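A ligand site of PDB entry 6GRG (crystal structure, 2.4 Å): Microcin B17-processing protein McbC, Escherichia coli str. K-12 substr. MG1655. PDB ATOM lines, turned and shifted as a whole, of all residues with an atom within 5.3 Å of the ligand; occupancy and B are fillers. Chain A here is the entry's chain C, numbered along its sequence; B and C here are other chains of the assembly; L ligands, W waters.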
ATOM      1  N   ARG A  82      11.997   7.029 -25.261  1.00  0.00           N
ATOM      2  CA  ARG A  82      13.072   7.262 -24.294  1.00  0.00           C
ATOM      3  C   ARG A  82      13.915   5.981 -24.236  1.00  0.00           C
ATOM      4  O   ARG A  82      13.373   4.867 -24.301  1.00  0.00           O
ATOM      5  CB  ARG A  82      12.477   7.678 -22.948  1.00  0.00           C
ATOM      6  CG  ARG A  82      13.470   7.910 -21.835  1.00  0.00           C
ATOM      7  CD  ARG A  82      12.796   8.297 -20.528  1.00  0.00           C
ATOM      8  NE  ARG A  82      11.826   7.319 -20.125  1.00  0.00           N
ATOM      9  CZ  ARG A  82      12.058   6.296 -19.295  1.00  0.00           C
ATOM     10  NH1 ARG A  82      13.268   6.132 -18.778  1.00  0.00           N
ATOM     11  NH2 ARG A  82      11.086   5.457 -18.998  1.00  0.00           N
ATOM     12  N   LEU A  83      15.247   6.150 -24.200  1.00  0.00           N
ATOM     13  CA  LEU A  83      16.173   5.054 -24.034  1.00  0.00           C
ATOM     14  C   LEU A  83      15.912   4.393 -22.687  1.00  0.00           C
ATOM     15  O   LEU A  83      15.499   5.071 -21.761  1.00  0.00           O
ATOM     16  CB  LEU A  83      17.609   5.580 -24.082  1.00  0.00           C
ATOM     17  CG  LEU A  83      18.164   5.918 -25.463  1.00  0.00           C
ATOM     18  CD1 LEU A  83      19.617   6.369 -25.337  1.00  0.00           C
ATOM     19  CD2 LEU A  83      18.038   4.750 -26.425  1.00  0.00           C
ATOM     20  N   PRO A  84      16.162   3.082 -22.522  1.00  0.00           N
ATOM     21  CA  PRO A  84      16.170   2.472 -21.197  1.00  0.00           C
ATOM     22  C   PRO A  84      17.229   3.147 -20.326  1.00  0.00           C
ATOM     23  O   PRO A  84      18.230   3.605 -20.849  1.00  0.00           O
ATOM     24  CB  PRO A  84      16.540   0.996 -21.464  1.00  0.00           C
ATOM     25  CG  PRO A  84      16.195   0.775 -22.919  1.00  0.00           C
ATOM     26  CD  PRO A  84      16.454   2.115 -23.589  1.00  0.00           C
ATOM     27  N   SER A  85      16.969   3.235 -19.016  1.00  0.00           N
ATOM     28  CA  SER A  85      17.910   3.828 -18.072  1.00  0.00           C
ATOM     29  C   SER A  85      19.126   2.914 -17.948  1.00  0.00           C
ATOM     30  O   SER A  85      18.945   1.743 -17.652  1.00  0.00           O
ATOM     31  CB  SER A  85      17.287   4.054 -16.710  1.00  0.00           C
ATOM     32  OG  SER A  85      16.075   4.756 -16.833  1.00  0.00           O
ATOM     33  N   ILE A  87      22.330   0.738 -16.876  1.00  0.00           N
ATOM     34  CA  ILE A  87      22.763   0.048 -15.669  1.00  0.00           C
ATOM     35  C   ILE A  87      24.066  -0.662 -15.988  1.00  0.00           C
ATOM     36  O   ILE A  87      24.392  -0.779 -17.142  1.00  0.00           O
ATOM     37  CB  ILE A  87      21.667  -0.884 -15.128  1.00  0.00           C
ATOM     38  CG1 ILE A  87      21.817  -1.139 -13.624  1.00  0.00           C
ATOM     39  CG2 ILE A  87      21.582  -2.181 -15.923  1.00  0.00           C
ATOM     40  CD1 ILE A  87      21.912   0.152 -12.786  1.00  0.00           C
ATOM     41  N   ASP A 178      24.050  -0.574  -3.572  1.00  0.00           N
ATOM     42  CA  ASP A 178      23.695  -1.239  -4.856  1.00  0.00           C
ATOM     43  C   ASP A 178      24.726  -0.905  -5.952  1.00  0.00           C
ATOM     44  O   ASP A 178      24.406  -0.935  -7.157  1.00  0.00           O
ATOM     45  CB  ASP A 178      22.281  -0.846  -5.292  1.00  0.00           C
ATOM     46  CG  ASP A 178      21.676  -1.708  -6.383  1.00  0.00           C
ATOM     47  OD1 ASP A 178      21.762  -2.937  -6.268  1.00  0.00           O
ATOM     48  OD2 ASP A 178      21.147  -1.135  -7.349  1.00  0.00           O
ATOM     49  N   ARG A 181      25.665  -3.343  -9.069  1.00  0.00           N
ATOM     50  CA  ARG A 181      24.702  -3.417 -10.178  1.00  0.00           C
ATOM     51  C   ARG A 181      24.848  -2.181 -11.062  1.00  0.00           C
ATOM     52  O   ARG A 181      24.740  -2.254 -12.275  1.00  0.00           O
ATOM     53  CB  ARG A 181      23.286  -3.447  -9.622  1.00  0.00           C
ATOM     54  CG  ARG A 181      22.194  -3.480 -10.685  1.00  0.00           C
ATOM     55  CD  ARG A 181      20.835  -3.701 -10.073  1.00  0.00           C
ATOM     56  NE  ARG A 181      19.796  -3.111 -10.902  1.00  0.00           N
ATOM     57  CZ  ARG A 181      19.303  -1.885 -10.745  1.00  0.00           C
ATOM     58  NH1 ARG A 181      19.693  -1.134  -9.726  1.00  0.00           N
ATOM     59  NH2 ARG A 181      18.420  -1.421 -11.607  1.00  0.00           N
ATOM     60  N   TYR A 218      15.692  17.088 -13.697  1.00  0.00           N
ATOM     61  CA  TYR A 218      16.354  15.901 -14.102  1.00  0.00           C
ATOM     62  C   TYR A 218      15.741  15.357 -15.405  1.00  0.00           C
ATOM     63  O   TYR A 218      16.426  14.696 -16.139  1.00  0.00           O
ATOM     64  CB  TYR A 218      16.463  14.871 -12.981  1.00  0.00           C
ATOM     65  CG  TYR A 218      15.214  14.165 -12.553  1.00  0.00           C
ATOM     66  CD1 TYR A 218      14.404  13.473 -13.444  1.00  0.00           C
ATOM     67  CD2 TYR A 218      14.902  14.075 -11.202  1.00  0.00           C
ATOM     68  CE1 TYR A 218      13.289  12.773 -13.018  1.00  0.00           C
ATOM     69  CE2 TYR A 218      13.776  13.394 -10.757  1.00  0.00           C
ATOM     70  CZ  TYR A 218      12.955  12.745 -11.668  1.00  0.00           C
ATOM     71  OH  TYR A 218      11.866  12.050 -11.216  1.00  0.00           O
ATOM     72  N   ARG A 233      20.663   7.193 -15.312  1.00  0.00           N
ATOM     73  CA  ARG A 233      19.714   6.580 -14.386  1.00  0.00           C
ATOM     74  C   ARG A 233      19.523   7.515 -13.185  1.00  0.00           C
ATOM     75  O   ARG A 233      20.477   7.850 -12.465  1.00  0.00           O
ATOM     76  CB  ARG A 233      20.170   5.168 -13.986  1.00  0.00           C
ATOM     77  CG  ARG A 233      19.238   4.467 -13.000  1.00  0.00           C
ATOM     78  CD  ARG A 233      19.570   3.011 -12.772  1.00  0.00           C
ATOM     79  NE  ARG A 233      19.282   2.145 -13.908  1.00  0.00           N
ATOM     80  CZ  ARG A 233      18.142   1.503 -14.119  1.00  0.00           C
ATOM     81  NH1 ARG A 233      17.153   1.614 -13.250  1.00  0.00           N
ATOM     82  NH2 ARG A 233      17.979   0.783 -15.221  1.00  0.00           N
ATOM     83  N   VAL A 234      18.292   7.976 -13.017  1.00  0.00           N
ATOM     84  CA  VAL A 234      17.921   8.690 -11.824  1.00  0.00           C
ATOM     85  C   VAL A 234      18.006   7.661 -10.687  1.00  0.00           C
ATOM     86  O   VAL A 234      17.776   6.482 -10.904  1.00  0.00           O
ATOM     87  CB  VAL A 234      16.552   9.363 -12.002  1.00  0.00           C
ATOM     88  CG1 VAL A 234      16.175  10.218 -10.794  1.00  0.00           C
ATOM     89  CG2 VAL A 234      16.502  10.216 -13.272  1.00  0.00           C
ATOM     90  N   TRP A 235      18.444   8.092  -9.499  1.00  0.00           N
ATOM     91  CA  TRP A 235      18.890   7.180  -8.443  1.00  0.00           C
ATOM     92  C   TRP A 235      18.506   7.700  -7.058  1.00  0.00           C
ATOM     93  O   TRP A 235      18.854   8.816  -6.706  1.00  0.00           O
ATOM     94  CB  TRP A 235      20.405   7.025  -8.548  1.00  0.00           C
ATOM     95  CG  TRP A 235      21.041   5.945  -7.716  1.00  0.00           C
ATOM     96  CD1 TRP A 235      21.672   6.090  -6.500  1.00  0.00           C
ATOM     97  CD2 TRP A 235      21.235   4.579  -8.107  1.00  0.00           C
ATOM     98  NE1 TRP A 235      22.233   4.899  -6.119  1.00  0.00           N
ATOM     99  CE2 TRP A 235      21.973   3.958  -7.088  1.00  0.00           C
ATOM    100  CE3 TRP A 235      20.867   3.833  -9.233  1.00  0.00           C
ATOM    101  CZ2 TRP A 235      22.304   2.603  -7.142  1.00  0.00           C
ATOM    102  CZ3 TRP A 235      21.202   2.487  -9.297  1.00  0.00           C
ATOM    103  CH2 TRP A 235      21.907   1.889  -8.253  1.00  0.00           C
ATOM    104  N   ALA A 236      17.835   6.863  -6.278  1.00  0.00           N
ATOM    105  CA  ALA A 236      17.395   7.201  -4.933  1.00  0.00           C
ATOM    106  C   ALA A 236      18.096   6.341  -3.882  1.00  0.00           C
ATOM    107  O   ALA A 236      17.898   6.571  -2.686  1.00  0.00           O
ATOM    108  CB  ALA A 236      15.894   7.062  -4.829  1.00  0.00           C
ATOM    109  N   GLY A 237      18.948   5.396  -4.308  1.00  0.00           N
ATOM    110  CA  GLY A 237      19.663   4.474  -3.411  1.00  0.00           C
ATOM    111  C   GLY A 237      20.966   5.042  -2.841  1.00  0.00           C
ATOM    112  O   GLY A 237      22.091   4.508  -3.087  1.00  0.00           O
ATOM    113  N   ILE A 258      17.838  13.883  -4.966  1.00  0.00           N
ATOM    114  CA  ILE A 258      18.011  12.844  -5.950  1.00  0.00           C
ATOM    115  C   ILE A 258      19.392  12.976  -6.622  1.00  0.00           C
ATOM    116  O   ILE A 258      19.972  14.061  -6.765  1.00  0.00           O
ATOM    117  CB  ILE A 258      16.825  12.837  -6.940  1.00  0.00           C
ATOM    118  CG1 ILE A 258      16.646  11.473  -7.615  1.00  0.00           C
ATOM    119  CG2 ILE A 258      16.956  13.945  -7.976  1.00  0.00           C
ATOM    120  CD1 ILE A 258      16.012  10.423  -6.745  1.00  0.00           C
ATOM    121  N   ARG B 117       6.763   1.487 -21.957  1.00  0.00           N
ATOM    122  CA  ARG B 117       7.866   2.341 -21.539  1.00  0.00           C
ATOM    123  C   ARG B 117       7.529   3.813 -21.829  1.00  0.00           C
ATOM    124  O   ARG B 117       7.586   4.261 -22.972  1.00  0.00           O
ATOM    125  CB  ARG B 117       9.158   1.901 -22.236  1.00  0.00           C
ATOM    126  CG  ARG B 117       9.711   0.572 -21.751  1.00  0.00           C
ATOM    127  CD  ARG B 117      11.225   0.537 -21.829  1.00  0.00           C
ATOM    128  NE  ARG B 117      11.816   1.718 -21.218  1.00  0.00           N
ATOM    129  CZ  ARG B 117      12.228   2.798 -21.889  1.00  0.00           C
ATOM    130  NH1 ARG B 117      12.263   2.787 -23.212  1.00  0.00           N
ATOM    131  NH2 ARG B 117      12.592   3.881 -21.238  1.00  0.00           N
ATOM    132  N   ARG B 118       7.209   4.560 -20.767  1.00  0.00           N
ATOM    133  CA  ARG B 118       6.808   5.973 -20.837  1.00  0.00           C
ATOM    134  C   ARG B 118       8.026   6.859 -21.048  1.00  0.00           C
ATOM    135  O   ARG B 118       9.147   6.457 -20.746  1.00  0.00           O
ATOM    136  CB  ARG B 118       6.074   6.400 -19.561  1.00  0.00           C
ATOM    137  CG  ARG B 118       4.839   5.553 -19.290  1.00  0.00           C
ATOM    138  CD  ARG B 118       4.102   5.973 -18.056  1.00  0.00           C
ATOM    139  NE  ARG B 118       3.475   4.829 -17.425  1.00  0.00           N
ATOM    140  CZ  ARG B 118       2.533   4.920 -16.495  1.00  0.00           C
ATOM    141  NH1 ARG B 118       2.038   6.103 -16.156  1.00  0.00           N
ATOM    142  NH2 ARG B 118       2.141   3.802 -15.894  1.00  0.00           N
ATOM    143  N   PRO B 121      10.939   8.530 -16.430  1.00  0.00           N
ATOM    144  CA  PRO B 121      11.248   7.432 -15.525  1.00  0.00           C
ATOM    145  C   PRO B 121      10.373   7.471 -14.256  1.00  0.00           C
ATOM    146  O   PRO B 121       9.539   8.353 -14.105  1.00  0.00           O
ATOM    147  CB  PRO B 121      12.739   7.635 -15.239  1.00  0.00           C
ATOM    148  CG  PRO B 121      12.960   9.114 -15.388  1.00  0.00           C
ATOM    149  CD  PRO B 121      11.958   9.574 -16.430  1.00  0.00           C
ATOM    150  N   SER B 122      10.556   6.489 -13.362  1.00  0.00           N
ATOM    151  CA  SER B 122       9.699   6.391 -12.167  1.00  0.00           C
ATOM    152  C   SER B 122      10.313   5.403 -11.172  1.00  0.00           C
ATOM    153  O   SER B 122      10.637   4.273 -11.545  1.00  0.00           O
ATOM    154  CB  SER B 122       8.294   5.959 -12.507  1.00  0.00           C
ATOM    155  OG  SER B 122       7.521   5.872 -11.315  1.00  0.00           O
ATOM    156  N   GLY B 123      10.472   5.851  -9.920  1.00  0.00           N
ATOM    157  CA  GLY B 123      10.856   4.993  -8.824  1.00  0.00           C
ATOM    158  C   GLY B 123      10.082   3.692  -8.876  1.00  0.00           C
ATOM    159  O   GLY B 123       8.834   3.709  -8.956  1.00  0.00           O
ATOM    160  N   GLY B 124      10.820   2.585  -8.954  1.00  0.00           N
ATOM    161  CA  GLY B 124      10.251   1.245  -8.923  1.00  0.00           C
ATOM    162  C   GLY B 124       9.363   0.915 -10.110  1.00  0.00           C
ATOM    163  O   GLY B 124       8.756  -0.164 -10.137  1.00  0.00           O
ATOM    164  N   ALA B 125       9.355   1.785 -11.125  1.00  0.00           N
ATOM    165  CA  ALA B 125       8.429   1.710 -12.268  1.00  0.00           C
ATOM    166  C   ALA B 125       6.973   1.668 -11.771  1.00  0.00           C
ATOM    167  O   ALA B 125       6.117   1.034 -12.403  1.00  0.00           O
ATOM    168  CB  ALA B 125       8.743   0.505 -13.138  1.00  0.00           C
ATOM    169  N   TYR B 127       4.940   4.491 -11.039  1.00  0.00           N
ATOM    170  CA  TYR B 127       4.104   5.485 -11.753  1.00  0.00           C
ATOM    171  C   TYR B 127       2.882   5.868 -10.931  1.00  0.00           C
ATOM    172  O   TYR B 127       1.760   5.653 -11.365  1.00  0.00           O
ATOM    173  CB  TYR B 127       3.738   4.959 -13.146  1.00  0.00           C
ATOM    174  CG  TYR B 127       4.944   4.876 -14.049  1.00  0.00           C
ATOM    175  CD1 TYR B 127       5.395   6.029 -14.667  1.00  0.00           C
ATOM    176  CD2 TYR B 127       5.691   3.722 -14.200  1.00  0.00           C
ATOM    177  CE1 TYR B 127       6.519   6.019 -15.482  1.00  0.00           C
ATOM    178  CE2 TYR B 127       6.821   3.691 -15.005  1.00  0.00           C
ATOM    179  CZ  TYR B 127       7.235   4.849 -15.640  1.00  0.00           C
ATOM    180  OH  TYR B 127       8.350   4.928 -16.402  1.00  0.00           O
ATOM    181  N   MET B 209       9.922  10.855  -4.204  1.00  0.00           N
ATOM    182  CA  MET B 209       9.966  10.342  -5.580  1.00  0.00           C
ATOM    183  C   MET B 209       8.677  10.704  -6.339  1.00  0.00           C
ATOM    184  O   MET B 209       8.750  11.023  -7.537  1.00  0.00           O
ATOM    185  CB  MET B 209      10.203   8.826  -5.631  1.00  0.00           C
ATOM    186  CG  MET B 209      11.490   8.338  -4.940  1.00  0.00           C
ATOM    187  SD  MET B 209      11.640   6.519  -5.003  1.00  0.00           S
ATOM    188  CE  MET B 209      12.254   6.152  -3.375  1.00  0.00           C
ATOM    189  N   MET B 212       8.575  14.567  -7.429  1.00  0.00           N
ATOM    190  CA  MET B 212       9.595  14.737  -8.473  1.00  0.00           C
ATOM    191  C   MET B 212       9.070  14.185  -9.808  1.00  0.00           C
ATOM    192  O   MET B 212       9.203  14.819 -10.855  1.00  0.00           O
ATOM    193  CB  MET B 212      10.916  14.053  -8.070  1.00  0.00           C
ATOM    194  CG  MET B 212      11.596  14.737  -6.849  1.00  0.00           C
ATOM    195  SD  MET B 212      13.312  14.264  -6.485  1.00  0.00           S
ATOM    196  CE  MET B 212      13.015  12.542  -6.066  1.00  0.00           C
ATOM    197  N   F6N C  64      17.513   1.695  -3.600  1.00  0.00           N
ATOM    198  CA1 F6N C  64      16.396   2.655  -3.526  1.00  0.00           C
ATOM    199  C2  F6N C  64      15.554   2.777  -4.754  1.00  0.00           C
ATOM    200  N2  F6N C  64      15.448   1.919  -5.718  1.00  0.00           N
ATOM    201  CA2 F6N C  64      14.556   2.431  -6.661  1.00  0.00           C
ATOM    202  C   F6N C  64      14.253   1.702  -7.988  1.00  0.00           C
ATOM    203  O   F6N C  64      13.450   2.182  -8.782  1.00  0.00           O
ATOM    204  C5  F6N C  64      14.141   3.674  -6.170  1.00  0.00           C
ATOM    205  O3  F6N C  64      14.772   3.870  -4.972  1.00  0.00           O
ATOM    206  N   GLY C  65      14.989   0.630  -8.281  1.00  0.00           N
ATOM    207  CA  GLY C  65      14.899  -0.065  -9.571  1.00  0.00           C
ATOM    208  C   GLY C  65      13.576  -0.788  -9.641  1.00  0.00           C
ATOM    209  O   GLY C  65      12.821  -0.709  -8.682  1.00  0.00           O
ATOM    210  N   SER C  66      13.305  -1.453 -10.784  1.00  0.00           N
ATOM    211  CA  SER C  66      12.155  -2.368 -10.969  1.00  0.00           C
ATOM    212  C   SER C  66      12.627  -3.837 -10.927  1.00  0.00           C
ATOM    213  O   SER C  66      13.754  -4.099 -11.314  1.00  0.00           O
ATOM    214  CB  SER C  66      11.465  -2.066 -12.269  1.00  0.00           C
ATOM    215  OG  SER C  66      11.992  -2.859 -13.320  1.00  0.00           O
HETATM  216  N1  LIG L   1      16.780   2.763 -10.635  1.00  0.00           N
HETATM  217  C1  LIG L   1      17.627   2.046  -9.853  1.00  0.00           C
HETATM  218  O1  LIG L   1      18.192   1.036 -10.323  1.00  0.00           O
HETATM  219  N2  LIG L   1      17.864   2.371  -8.559  1.00  0.00           N
HETATM  220  C2  LIG L   1      17.305   3.452  -7.973  1.00  0.00           C
HETATM  221  O2  LIG L   1      17.559   3.742  -6.779  1.00  0.00           O
HETATM  222  C3  LIG L   1      16.371   4.290  -8.757  1.00  0.00           C
HETATM  223  N3  LIG L   1      15.757   5.351  -8.214  1.00  0.00           N
HETATM  224  C4  LIG L   1      14.908   6.106  -8.963  1.00  0.00           C
HETATM  225  C5  LIG L   1      14.306   7.223  -8.394  1.00  0.00           C
HETATM  226  C6  LIG L   1      13.450   8.010  -9.144  1.00  0.00           C
HETATM  227  C7  LIG L   1      12.798   9.211  -8.530  1.00  0.00           C
HETATM  228  C8  LIG L   1      13.174   7.667 -10.559  1.00  0.00           C
HETATM  229  C9  LIG L   1      12.231   8.516 -11.345  1.00  0.00           C
HETATM  230  C10 LIG L   1      13.759   6.553 -11.142  1.00  0.00           C
HETATM  231  C11 LIG L   1      14.635   5.754 -10.399  1.00  0.00           C
HETATM  232  N4  LIG L   1      15.283   4.611 -10.959  1.00  0.00           N
HETATM  233  C12 LIG L   1      16.142   3.861 -10.156  1.00  0.00           C
HETATM  234  C13 LIG L   1      15.063   4.189 -12.346  1.00  0.00           C
HETATM  235  C14 LIG L   1      13.737   3.428 -12.429  1.00  0.00           C
HETATM  236  O3  LIG L   1      13.881   2.180 -11.709  1.00  0.00           O
HETATM  237  C15 LIG L   1      13.371   3.313 -13.914  1.00  0.00           C
HETATM  238  O4  LIG L   1      13.008   4.602 -14.443  1.00  0.00           O
HETATM  239  C16 LIG L   1      12.185   2.374 -14.139  1.00  0.00           C
HETATM  240  O5  LIG L   1      12.507   1.063 -13.671  1.00  0.00           O
HETATM  241  C17 LIG L   1      11.786   2.281 -15.600  1.00  0.00           C
HETATM  242  O6  LIG L   1      12.899   1.827 -16.387  1.00  0.00           O
HETATM  243  P1  LIG L   1      13.382   2.726 -17.614  1.00  0.00           P
HETATM  244  O7  LIG L   1      13.683   4.080 -16.985  1.00  0.00           O
HETATM  245  O8  LIG L   1      14.584   1.957 -18.079  1.00  0.00           O
HETATM  246  O9  LIG L   1      12.178   2.748 -18.545  1.00  0.00           O
HETATM  247  O   HOH W   1      15.827   0.048 -17.065  1.00  0.00           O
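O of Ser 85 lies within hydrogen-bond range of NH2 of Arg 233, 2.8 Å away. The guanidinium group (NH1) of Arg 181 lies within salt-bridge range of the side-chain carboxylate (OD2) of Asp 178 (2.8 Å). The backbone carbonyl oxygen (O) of Arg 82 sits at hydrogen-bond distance from the guanidinium group (NH1) of Arg 117 of chain B (2.6 Å). O of Arg 118 of chain B is in hydrogen-bond range of NH2 of Arg 82, at 2.8 Å. NH2 of Arg 117 of chain B is in hydrogen-bond range of O of Leu 83. The backbone NH (N) of Gly 124 of chain B lies within hydrogen-bond range of O of F6N 64 of chain C, 2.7 Å away. N of Tyr 127 of chain B sits at hydrogen-bond distance from OG of Ser 122 of chain B (2.9 Å). O of Gly 237 is in hydrogen-bond range of NE1 of Trp 235.
The backbone carbonyl oxygen (O) of Val 234 lies close to a nitrogen (N4) of the ligand. The backbone NH of Gly 65 of chain C lies close to a nitrogen (N2) of the ligand (3.4 Å). Pro 84 touches the ligand (CA to O8, 3.5 Å). Tyr 218 touches the ligand. CE3 of Trp 235 touches N2 of the ligand, 3.4 Å away. CD1 of Ile 258 touches C7 of the ligand (3.9 Å). CB of Pro 121 of chain B touches O4 of the ligand, at 3.1 Å. N of Gly 123 of chain B touches C8 of the ligand, at 3.3 Å. Ala 125 of chain B touches the ligand (CB to O5, 3.8 Å). Met 209 of chain B touches the ligand. CB of Ser 66 of chain C touches O5 of the ligand (3.6 Å). Hydrophobic or aromatic side chains within 4 Å of the ligand: Val 234, Trp 235, Ala 236, Ile 258, Pro 121 of chain B, Ala 125 of chain B and Met 209 of chain B. 20 residues have an atom within 4 Å of the ligand: Arg 82, Pro 84, Ser 85, Arg 181, Tyr 218, Arg 233, Val 234, Trp 235, Ala 236, Gly 237, Ile 258, Arg 117 of chain B, Pro 121 of chain B, Ser 122 of chain B, Gly 123 of chain B, Ala 125 of chain B, Met 209 of chain B, F6N 64 of chain C, Gly 65 of chain C and Ser 66 of chain C. Along chain A the residues within 4 Å of the ligand span positions 82 to 258.
Water W1 lies within hydrogen-bond range of an oxygen (O8) of the ligand (2.5 Å) and the guanidinium group (NH2) of Arg 233 (2.9 Å).
An oxygen (O8) of the ligand sits at hydrogen-bond distance from the backbone NH (N) of Ser 85, at 2.9 Å. The side-chain hydroxyl of Ser 85 is in hydrogen-bond range of an oxygen (O7) of the ligand (2.5 Å). An oxygen (O1) of the ligand lies within hydrogen-bond range of the guanidinium group (NH1) of Arg 181, 2.7 Å away. An oxygen (O7) of the ligand lies within salt-bridge range of the guanidinium group (NH1) of Arg 82, at 2.8 Å. The guanidinium group (NH1) of Arg 233 lies within hydrogen-bond range of a nitrogen (N1) of the ligand (2.9 Å). NE of Arg 117 of chain B is in salt-bridge range of O9 of the ligand, 2.9 Å away. An oxygen (O3) of the ligand lies within hydrogen-bond range of O of F6N 64 of chain C (3.0 Å). An oxygen (O2) of the ligand lies within hydrogen-bond range of the backbone NH (N) of Ala 236. The backbone NH (N) of Ser 122 of chain B is in hydrogen-bond range of an oxygen (O4) of the ligand (3.3 Å). N of Gly 237 sits at hydrogen-bond distance from O2 of the ligand (3.3 Å).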
